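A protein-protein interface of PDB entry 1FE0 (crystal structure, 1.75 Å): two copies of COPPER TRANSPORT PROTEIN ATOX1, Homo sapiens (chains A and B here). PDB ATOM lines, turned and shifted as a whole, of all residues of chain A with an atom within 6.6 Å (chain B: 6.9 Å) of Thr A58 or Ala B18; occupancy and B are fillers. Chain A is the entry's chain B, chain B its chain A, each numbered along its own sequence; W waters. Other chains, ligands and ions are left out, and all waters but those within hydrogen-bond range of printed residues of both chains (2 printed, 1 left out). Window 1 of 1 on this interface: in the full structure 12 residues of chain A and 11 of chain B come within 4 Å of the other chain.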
ATOM      1  N   VAL A   8      21.810 -25.531  20.406  1.00  0.00           N
ATOM      2  CA  VAL A   8      22.368 -24.324  19.794  1.00  0.00           C
ATOM      3  C   VAL A   8      21.898 -23.164  20.664  1.00  0.00           C
ATOM      4  O   VAL A   8      20.698 -22.939  20.803  1.00  0.00           O
ATOM      5  CB  VAL A   8      21.853 -24.126  18.351  1.00  0.00           C
ATOM      6  CG1 VAL A   8      22.495 -22.891  17.742  1.00  0.00           C
ATOM      7  CG2 VAL A   8      22.165 -25.358  17.509  1.00  0.00           C
ATOM      8  N   CYS A  15      18.480 -15.106  15.914  1.00  0.00           N
ATOM      9  CA  CYS A  15      19.413 -16.224  16.062  1.00  0.00           C
ATOM     10  C   CYS A  15      18.827 -17.437  15.345  1.00  0.00           C
ATOM     11  O   CYS A  15      19.534 -18.160  14.640  1.00  0.00           O
ATOM     12  CB  CYS A  15      19.623 -16.585  17.544  1.00  0.00           C
ATOM     13  SG  CYS A  15      20.715 -15.488  18.505  1.00  0.00           S
ATOM     14  N   ALA A  18      18.958 -17.138  11.506  1.00  0.00           N
ATOM     15  CA  ALA A  18      20.308 -17.406  11.010  1.00  0.00           C
ATOM     16  C   ALA A  18      20.589 -18.903  10.950  1.00  0.00           C
ATOM     17  O   ALA A  18      21.218 -19.382  10.003  1.00  0.00           O
ATOM     18  CB  ALA A  18      21.344 -16.698  11.887  1.00  0.00           C
ATOM     19  N   VAL A  19      20.135 -19.641  11.962  1.00  0.00           N
ATOM     20  CA  VAL A  19      20.320 -21.090  11.978  1.00  0.00           C
ATOM     21  C   VAL A  19      19.559 -21.646  10.775  1.00  0.00           C
ATOM     22  O   VAL A  19      20.047 -22.519  10.061  1.00  0.00           O
ATOM     23  CB  VAL A  19      19.767 -21.713  13.287  1.00  0.00           C
ATOM     24  CG1 VAL A  19      19.683 -23.234  13.161  1.00  0.00           C
ATOM     25  CG2 VAL A  19      20.675 -21.346  14.455  1.00  0.00           C
ATOM     26  N   SER A  20      18.360 -21.120  10.548  1.00  0.00           N
ATOM     27  CA  SER A  20      17.546 -21.555   9.417  1.00  0.00           C
ATOM     28  C   SER A  20      18.278 -21.320   8.093  1.00  0.00           C
ATOM     29  O   SER A  20      18.294 -22.187   7.214  1.00  0.00           O
ATOM     30  CB  SER A  20      16.219 -20.794   9.397  1.00  0.00           C
ATOM     31  OG  SER A  20      15.480 -21.121   8.240  1.00  0.00           O
ATOM     32  N   VAL A  22      21.584 -21.085   7.409  1.00  0.00           N
ATOM     33  CA  VAL A  22      22.725 -21.950   7.126  1.00  0.00           C
ATOM     34  C   VAL A  22      22.258 -23.359   6.778  1.00  0.00           C
ATOM     35  O   VAL A  22      22.872 -24.027   5.946  1.00  0.00           O
ATOM     36  CB  VAL A  22      23.755 -22.000   8.302  1.00  0.00           C
ATOM     37  CG1 VAL A  22      24.206 -20.588   8.648  1.00  0.00           C
ATOM     38  CG2 VAL A  22      23.168 -22.697   9.515  1.00  0.00           C
ATOM     39  N   ALA A  53      29.322 -29.060  11.765  1.00  0.00           N
ATOM     40  CA  ALA A  53      30.138 -28.009  11.165  1.00  0.00           C
ATOM     41  C   ALA A  53      29.264 -26.887  10.622  1.00  0.00           C
ATOM     42  O   ALA A  53      29.574 -25.704  10.799  1.00  0.00           O
ATOM     43  CB  ALA A  53      30.992 -28.590  10.047  1.00  0.00           C
ATOM     44  N   THR A  54      28.173 -27.259   9.959  1.00  0.00           N
ATOM     45  CA  THR A  54      27.261 -26.273   9.393  1.00  0.00           C
ATOM     46  C   THR A  54      26.667 -25.398  10.489  1.00  0.00           C
ATOM     47  O   THR A  54      26.630 -24.177  10.367  1.00  0.00           O
ATOM     48  CB  THR A  54      26.123 -26.958   8.613  1.00  0.00           C
ATOM     49  OG1 THR A  54      26.673 -27.639   7.478  1.00  0.00           O
ATOM     50  CG2 THR A  54      25.099 -25.933   8.138  1.00  0.00           C
ATOM     51  N   LEU A  55      26.205 -26.020  11.566  1.00  0.00           N
ATOM     52  CA  LEU A  55      25.625 -25.252  12.661  1.00  0.00           C
ATOM     53  C   LEU A  55      26.654 -24.326  13.302  1.00  0.00           C
ATOM     54  O   LEU A  55      26.331 -23.201  13.678  1.00  0.00           O
ATOM     55  CB  LEU A  55      25.032 -26.194  13.714  1.00  0.00           C
ATOM     56  CG  LEU A  55      23.758 -26.927  13.282  1.00  0.00           C
ATOM     57  CD1 LEU A  55      23.385 -27.963  14.339  1.00  0.00           C
ATOM     58  CD2 LEU A  55      22.615 -25.918  13.081  1.00  0.00           C
ATOM     59  N   LYS A  56      27.896 -24.787  13.415  1.00  0.00           N
ATOM     60  CA  LYS A  56      28.941 -23.966  14.018  1.00  0.00           C
ATOM     61  C   LYS A  56      29.269 -22.719  13.193  1.00  0.00           C
ATOM     62  O   LYS A  56      29.854 -21.762  13.713  1.00  0.00           O
ATOM     63  CB  LYS A  56      30.209 -24.796  14.248  1.00  0.00           C
ATOM     64  CG  LYS A  56      30.143 -25.723  15.468  1.00  0.00           C
ATOM     65  CD  LYS A  56      31.382 -26.609  15.538  1.00  0.00           C
ATOM     66  CE  LYS A  56      31.420 -27.478  16.796  1.00  0.00           C
ATOM     67  NZ  LYS A  56      31.657 -26.688  18.038  1.00  0.00           N
ATOM     68  N   LYS A  57      28.882 -22.714  11.918  1.00  0.00           N
ATOM     69  CA  LYS A  57      29.142 -21.564  11.048  1.00  0.00           C
ATOM     70  C   LYS A  57      28.396 -20.319  11.513  1.00  0.00           C
ATOM     71  O   LYS A  57      28.763 -19.193  11.172  1.00  0.00           O
ATOM     72  CB  LYS A  57      28.734 -21.872   9.602  1.00  0.00           C
ATOM     73  CG  LYS A  57      29.658 -22.835   8.880  1.00  0.00           C
ATOM     74  CD  LYS A  57      29.192 -23.053   7.445  1.00  0.00           C
ATOM     75  CE  LYS A  57      30.117 -24.006   6.708  1.00  0.00           C
ATOM     76  NZ  LYS A  57      29.677 -24.206   5.300  1.00  0.00           N
ATOM     77  N   THR A  58      27.339 -20.532  12.286  1.00  0.00           N
ATOM     78  CA  THR A  58      26.529 -19.437  12.804  1.00  0.00           C
ATOM     79  C   THR A  58      27.296 -18.609  13.822  1.00  0.00           C
ATOM     80  O   THR A  58      26.953 -17.454  14.073  1.00  0.00           O
ATOM     81  CB  THR A  58      25.275 -19.958  13.516  1.00  0.00           C
ATOM     82  OG1 THR A  58      25.671 -20.788  14.614  1.00  0.00           O
ATOM     83  CG2 THR A  58      24.406 -20.758  12.561  1.00  0.00           C
ATOM     84  N   GLY A  59      28.325 -19.206  14.416  1.00  0.00           N
ATOM     85  CA  GLY A  59      29.101 -18.513  15.427  1.00  0.00           C
ATOM     86  C   GLY A  59      28.538 -18.790  16.809  1.00  0.00           C
ATOM     87  O   GLY A  59      29.038 -18.282  17.812  1.00  0.00           O
ATOM     88  N   LYS A  60      27.489 -19.604  16.855  1.00  0.00           N
ATOM     89  CA  LYS A  60      26.829 -19.972  18.107  1.00  0.00           C
ATOM     90  C   LYS A  60      27.505 -21.189  18.739  1.00  0.00           C
ATOM     91  O   LYS A  60      28.233 -21.918  18.069  1.00  0.00           O
ATOM     92  CB  LYS A  60      25.361 -20.307  17.838  1.00  0.00           C
ATOM     93  CG  LYS A  60      24.560 -19.181  17.187  1.00  0.00           C
ATOM     94  CD  LYS A  60      23.734 -18.407  18.209  1.00  0.00           C
ATOM     95  CE  LYS A  60      24.603 -17.764  19.278  1.00  0.00           C
ATOM     96  NZ  LYS A  60      23.779 -17.005  20.261  1.00  0.00           N
ATOM     97  N   THR A  61      27.273 -21.395  20.031  1.00  0.00           N
ATOM     98  CA  THR A  61      27.835 -22.552  20.722  1.00  0.00           C
ATOM     99  C   THR A  61      26.930 -23.722  20.381  1.00  0.00           C
ATOM    100  O   THR A  61      25.720 -23.665  20.602  1.00  0.00           O
ATOM    101  CB  THR A  61      27.858 -22.345  22.247  1.00  0.00           C
ATOM    102  OG1 THR A  61      28.781 -21.295  22.562  1.00  0.00           O
ATOM    103  CG2 THR A  61      28.297 -23.618  22.958  1.00  0.00           C
ATOM    104  N   VAL A  62      27.517 -24.785  19.842  1.00  0.00           N
ATOM    105  CA  VAL A  62      26.743 -25.946  19.429  1.00  0.00           C
ATOM    106  C   VAL A  62      27.234 -27.244  20.057  1.00  0.00           C
ATOM    107  O   VAL A  62      28.438 -27.484  20.145  1.00  0.00           O
ATOM    108  CB  VAL A  62      26.802 -26.111  17.892  1.00  0.00           C
ATOM    109  CG1 VAL A  62      25.945 -27.297  17.450  1.00  0.00           C
ATOM    110  CG2 VAL A  62      26.345 -24.828  17.216  1.00  0.00           C
ATOM    111  N   GLY B  13      22.497  -9.476  22.069  1.00  0.00           N
ATOM    112  CA  GLY B  13      23.907  -9.601  22.380  1.00  0.00           C
ATOM    113  C   GLY B  13      24.479 -10.900  21.840  1.00  0.00           C
ATOM    114  O   GLY B  13      25.634 -10.951  21.418  1.00  0.00           O
ATOM    115  N   GLY B  14      23.666 -11.952  21.853  1.00  0.00           N
ATOM    116  CA  GLY B  14      24.110 -13.238  21.344  1.00  0.00           C
ATOM    117  C   GLY B  14      24.482 -13.167  19.873  1.00  0.00           C
ATOM    118  O   GLY B  14      25.384 -13.879  19.425  1.00  0.00           O
ATOM    119  N   CYS B  15      23.787 -12.313  19.121  1.00  0.00           N
ATOM    120  CA  CYS B  15      24.065 -12.145  17.698  1.00  0.00           C
ATOM    121  C   CYS B  15      25.439 -11.507  17.508  1.00  0.00           C
ATOM    122  O   CYS B  15      26.191 -11.881  16.609  1.00  0.00           O
ATOM    123  CB  CYS B  15      23.004 -11.257  17.030  1.00  0.00           C
ATOM    124  SG  CYS B  15      21.442 -12.071  16.563  1.00  0.00           S
ATOM    125  N   ALA B  16      25.754 -10.528  18.347  1.00  0.00           N
ATOM    126  CA  ALA B  16      27.039  -9.848  18.262  1.00  0.00           C
ATOM    127  C   ALA B  16      28.158 -10.805  18.645  1.00  0.00           C
ATOM    128  O   ALA B  16      29.226 -10.811  18.030  1.00  0.00           O
ATOM    129  CB  ALA B  16      27.050  -8.625  19.181  1.00  0.00           C
ATOM    130  N   GLU B  17      27.912 -11.619  19.665  1.00  0.00           N
ATOM    131  CA  GLU B  17      28.913 -12.572  20.115  1.00  0.00           C
ATOM    132  C   GLU B  17      29.222 -13.578  19.012  1.00  0.00           C
ATOM    133  O   GLU B  17      30.380 -13.964  18.819  1.00  0.00           O
ATOM    134  CB  GLU B  17      28.425 -13.296  21.373  1.00  0.00           C
ATOM    135  CG  GLU B  17      29.452 -14.247  21.967  1.00  0.00           C
ATOM    136  CD  GLU B  17      29.106 -14.675  23.381  1.00  0.00           C
ATOM    137  OE1 GLU B  17      28.012 -15.244  23.581  1.00  0.00           O
ATOM    138  OE2 GLU B  17      29.933 -14.440  24.289  1.00  0.00           O
ATOM    139  N   ALA B  18      28.188 -14.001  18.289  1.00  0.00           N
ATOM    140  CA  ALA B  18      28.359 -14.959  17.201  1.00  0.00           C
ATOM    141  C   ALA B  18      29.248 -14.355  16.119  1.00  0.00           C
ATOM    142  O   ALA B  18      30.087 -15.037  15.539  1.00  0.00           O
ATOM    143  CB  ALA B  18      27.001 -15.348  16.617  1.00  0.00           C
ATOM    144  N   VAL B  19      29.055 -13.069  15.842  1.00  0.00           N
ATOM    145  CA  VAL B  19      29.872 -12.389  14.842  1.00  0.00           C
ATOM    146  C   VAL B  19      31.324 -12.360  15.319  1.00  0.00           C
ATOM    147  O   VAL B  19      32.256 -12.622  14.555  1.00  0.00           O
ATOM    148  CB  VAL B  19      29.377 -10.945  14.621  1.00  0.00           C
ATOM    149  CG1 VAL B  19      30.382 -10.162  13.782  1.00  0.00           C
ATOM    150  CG2 VAL B  19      28.020 -10.977  13.924  1.00  0.00           C
ATOM    151  N   SER B  20      31.508 -12.043  16.595  1.00  0.00           N
ATOM    152  CA  SER B  20      32.836 -11.987  17.189  1.00  0.00           C
ATOM    153  C   SER B  20      33.554 -13.327  17.088  1.00  0.00           C
ATOM    154  O   SER B  20      34.752 -13.383  16.810  1.00  0.00           O
ATOM    155  CB  SER B  20      32.733 -11.582  18.660  1.00  0.00           C
ATOM    156  OG  SER B  20      34.018 -11.529  19.256  1.00  0.00           O
ATOM    157  N   ARG B  21      32.820 -14.411  17.310  1.00  0.00           N
ATOM    158  CA  ARG B  21      33.433 -15.728  17.255  1.00  0.00           C
ATOM    159  C   ARG B  21      33.901 -16.140  15.869  1.00  0.00           C
ATOM    160  O   ARG B  21      34.992 -16.687  15.730  1.00  0.00           O
ATOM    161  CB  ARG B  21      32.482 -16.776  17.825  1.00  0.00           C
ATOM    162  CG  ARG B  21      32.257 -16.598  19.309  1.00  0.00           C
ATOM    163  CD  ARG B  21      31.453 -17.735  19.893  1.00  0.00           C
ATOM    164  NE  ARG B  21      31.230 -17.548  21.322  1.00  0.00           N
ATOM    165  CZ  ARG B  21      30.496 -18.364  22.065  1.00  0.00           C
ATOM    166  NH1 ARG B  21      29.921 -19.417  21.505  1.00  0.00           N
ATOM    167  NH2 ARG B  21      30.331 -18.126  23.360  1.00  0.00           N
ATOM    168  N   VAL B  22      33.095 -15.882  14.842  1.00  0.00           N
ATOM    169  CA  VAL B  22      33.513 -16.261  13.497  1.00  0.00           C
ATOM    170  C   VAL B  22      34.686 -15.403  13.033  1.00  0.00           C
ATOM    171  O   VAL B  22      35.555 -15.881  12.303  1.00  0.00           O
ATOM    172  CB  VAL B  22      32.357 -16.162  12.473  1.00  0.00           C
ATOM    173  CG1 VAL B  22      31.197 -17.045  12.922  1.00  0.00           C
ATOM    174  CG2 VAL B  22      31.916 -14.717  12.298  1.00  0.00           C
ATOM    175  N   LEU B  23      34.725 -14.142  13.456  1.00  0.00           N
ATOM    176  CA  LEU B  23      35.834 -13.274  13.063  1.00  0.00           C
ATOM    177  C   LEU B  23      37.108 -13.709  13.785  1.00  0.00           C
ATOM    178  O   LEU B  23      38.201 -13.652  13.220  1.00  0.00           O
ATOM    179  CB  LEU B  23      35.519 -11.804  13.377  1.00  0.00           C
ATOM    180  CG  LEU B  23      34.427 -11.160  12.512  1.00  0.00           C
ATOM    181  CD1 LEU B  23      34.247  -9.695  12.900  1.00  0.00           C
ATOM    182  CD2 LEU B  23      34.807 -11.266  11.039  1.00  0.00           C
ATOM    183  N   ILE B  33      31.977  -3.989  17.237  1.00  0.00           N
ATOM    184  CA  ILE B  33      30.603  -4.307  16.894  1.00  0.00           C
ATOM    185  C   ILE B  33      29.663  -3.346  17.596  1.00  0.00           C
ATOM    186  O   ILE B  33      29.796  -3.097  18.794  1.00  0.00           O
ATOM    187  CB  ILE B  33      30.274  -5.760  17.295  1.00  0.00           C
ATOM    188  CG1 ILE B  33      31.204  -6.717  16.540  1.00  0.00           C
ATOM    189  CG2 ILE B  33      28.811  -6.070  16.997  1.00  0.00           C
ATOM    190  CD1 ILE B  33      31.087  -8.174  16.957  1.00  0.00           C
ATOM    191  N   LYS B  57      28.491 -16.373   6.100  1.00  0.00           N
ATOM    192  CA  LYS B  57      28.337 -17.762   6.509  1.00  0.00           C
ATOM    193  C   LYS B  57      27.598 -17.927   7.832  1.00  0.00           C
ATOM    194  O   LYS B  57      27.104 -19.014   8.132  1.00  0.00           O
ATOM    195  CB  LYS B  57      29.704 -18.452   6.566  1.00  0.00           C
ATOM    196  CG  LYS B  57      30.307 -18.677   5.188  1.00  0.00           C
ATOM    197  CD  LYS B  57      31.698 -19.291   5.253  1.00  0.00           C
ATOM    198  CE  LYS B  57      32.241 -19.537   3.852  1.00  0.00           C
ATOM    199  NZ  LYS B  57      33.644 -20.037   3.870  1.00  0.00           N
ATOM    200  N   THR B  58      27.503 -16.848   8.605  1.00  0.00           N
ATOM    201  CA  THR B  58      26.815 -16.884   9.896  1.00  0.00           C
ATOM    202  C   THR B  58      25.309 -17.044   9.725  1.00  0.00           C
ATOM    203  O   THR B  58      24.603 -17.377  10.674  1.00  0.00           O
ATOM    204  CB  THR B  58      27.043 -15.593  10.707  1.00  0.00           C
ATOM    205  OG1 THR B  58      26.416 -14.488  10.039  1.00  0.00           O
ATOM    206  CG2 THR B  58      28.530 -15.316  10.868  1.00  0.00           C
ATOM    207  N   GLY B  59      24.818 -16.796   8.517  1.00  0.00           N
ATOM    208  CA  GLY B  59      23.393 -16.911   8.274  1.00  0.00           C
ATOM    209  C   GLY B  59      22.668 -15.604   8.527  1.00  0.00           C
ATOM    210  O   GLY B  59      21.441 -15.537   8.443  1.00  0.00           O
ATOM    211  N   LYS B  60      23.425 -14.556   8.845  1.00  0.00           N
ATOM    212  CA  LYS B  60      22.828 -13.247   9.096  1.00  0.00           C
ATOM    213  C   LYS B  60      22.852 -12.422   7.817  1.00  0.00           C
ATOM    214  O   LYS B  60      23.656 -12.673   6.923  1.00  0.00           O
ATOM    215  CB  LYS B  60      23.593 -12.507  10.203  1.00  0.00           C
ATOM    216  CG  LYS B  60      23.684 -13.280  11.502  1.00  0.00           C
ATOM    217  CD  LYS B  60      24.204 -12.418  12.647  1.00  0.00           C
ATOM    218  CE  LYS B  60      24.477 -13.269  13.890  1.00  0.00           C
ATOM    219  NZ  LYS B  60      23.305 -14.115  14.241  1.00  0.00           N
HETATM  220  O   HOH W   1      27.655 -18.874  22.460  1.00  0.00           O
HETATM  221  O   HOH W   2      24.372 -16.651  13.201  1.00  0.00           O
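The guanidinium group (NH1) of Arg B21 sits at hydrogen-bond distance from the side-chain hydroxyl (OG1) of Thr A61 (2.4 Å).
O of Lys A57 sits close to O of Lys B57 (3.5 Å).
The side-chain amino group (NZ) of Lys B60 lies close to the side-chain sulfur (SG) of Cys B15 (3.6 Å).
The guanidinium group (NH2) of Arg B21 lies within salt-bridge range of the side-chain carboxylate (OE1) of Glu B17 (3.7 Å).
The side-chain hydroxyl (OG1) of Thr B58 is in hydrogen-bond range of the backbone NH (N) of Lys B60, at 3.2 Å.
OG1 of Thr A58 sits at hydrogen-bond distance from O of Leu A55 (2.7 Å).
The backbone NH (N) of Lys A60 sits at hydrogen-bond distance from the side-chain hydroxyl (OG1) of Thr A58, at 3.1 Å.
SG of Cys B15 touches SG of Cys A15, 3.997 Å away.
Thr B58 touches Ala A18 (O to CB, 3.5 Å).
Thr B58 touches Val A22.
Val A22 touches Gly B59 (CG1 to CA, 3.8 Å).
Lys A57 touches Val B22.
Lys A57 touches Thr B58 (O to CA, 3.3 Å).
Thr A58 touches Ala B18 (O to CB, 3.3 Å).
Thr A58 touches Thr B58.
Gly A59 touches Ala B18.
O of Gly A59 touches CD of Arg B21, 3.2 Å away.
Ser A20 touches none of the printed residues of chain B.
Printed residues of chain B within 4 Å of Val A22: Lys B57 (3.3 Å), Thr B58 (3.8 Å) and Gly B59 (3.8 Å).
Of chain B, only Ala B18 (3.3 Å) and Thr B58 (3.5 Å) come within 4 Å of Thr A58.
Ala B16 touches none of the printed residues of chain A.
Of chain A, only Thr A58 and Gly A59 come within 4 Å of Ala B18.
Of the printed residues of chain A, Thr B58 touches Ala A18 (3.5 Å), Val A22 (3.8 Å), Lys A57 (3.3 Å) and Thr A58 (3.5 Å).
The nearest printed residue of chain A that does not touch Gly B14 is Cys A15 (4.6 Å).
Of the 16 printed residues of chain A, 8 touch a printed residue of chain B.
Hydrophobic or aromatic side chains of chain A within 4 Å of the printed part of chain B: Ala A18 and Val A22.
Of the 16 printed residues of chain B, 8 touch a printed residue of chain A.
Among the printed residues, 16 pairs touch across the chains.
Among the printed residues, no Asp or Glu carboxylate lies within 4 Å of a Lys or Arg side-chain nitrogen of the other chain.
Cys B15 touches its own counterpart, Cys A15.
Ala A18 touches Thr B58, and with the chains exchanged Thr A58 touches Ala B18.
Val A22 touches Thr B58, but with the chains exchanged Thr A58 does not touch Val B22 (4.3 Å).
Thr A58 touches its own counterpart, Thr B58.
9 positions are printed for both chains.
Of the 16 pairs that touch across the chains among the printed residues, 11 have their exchanged pair printed and touching as well.
Water W1 bridges NH1 of Arg B21 and OG1 of Thr A61.
Water W2 lies within hydrogen-bond range of the backbone carbonyl oxygen of Thr B58 (2.6 Å), the backbone carbonyl oxygen of Thr A58 (2.8 Å) and the side-chain amino group of Lys B60 (2.9 Å).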
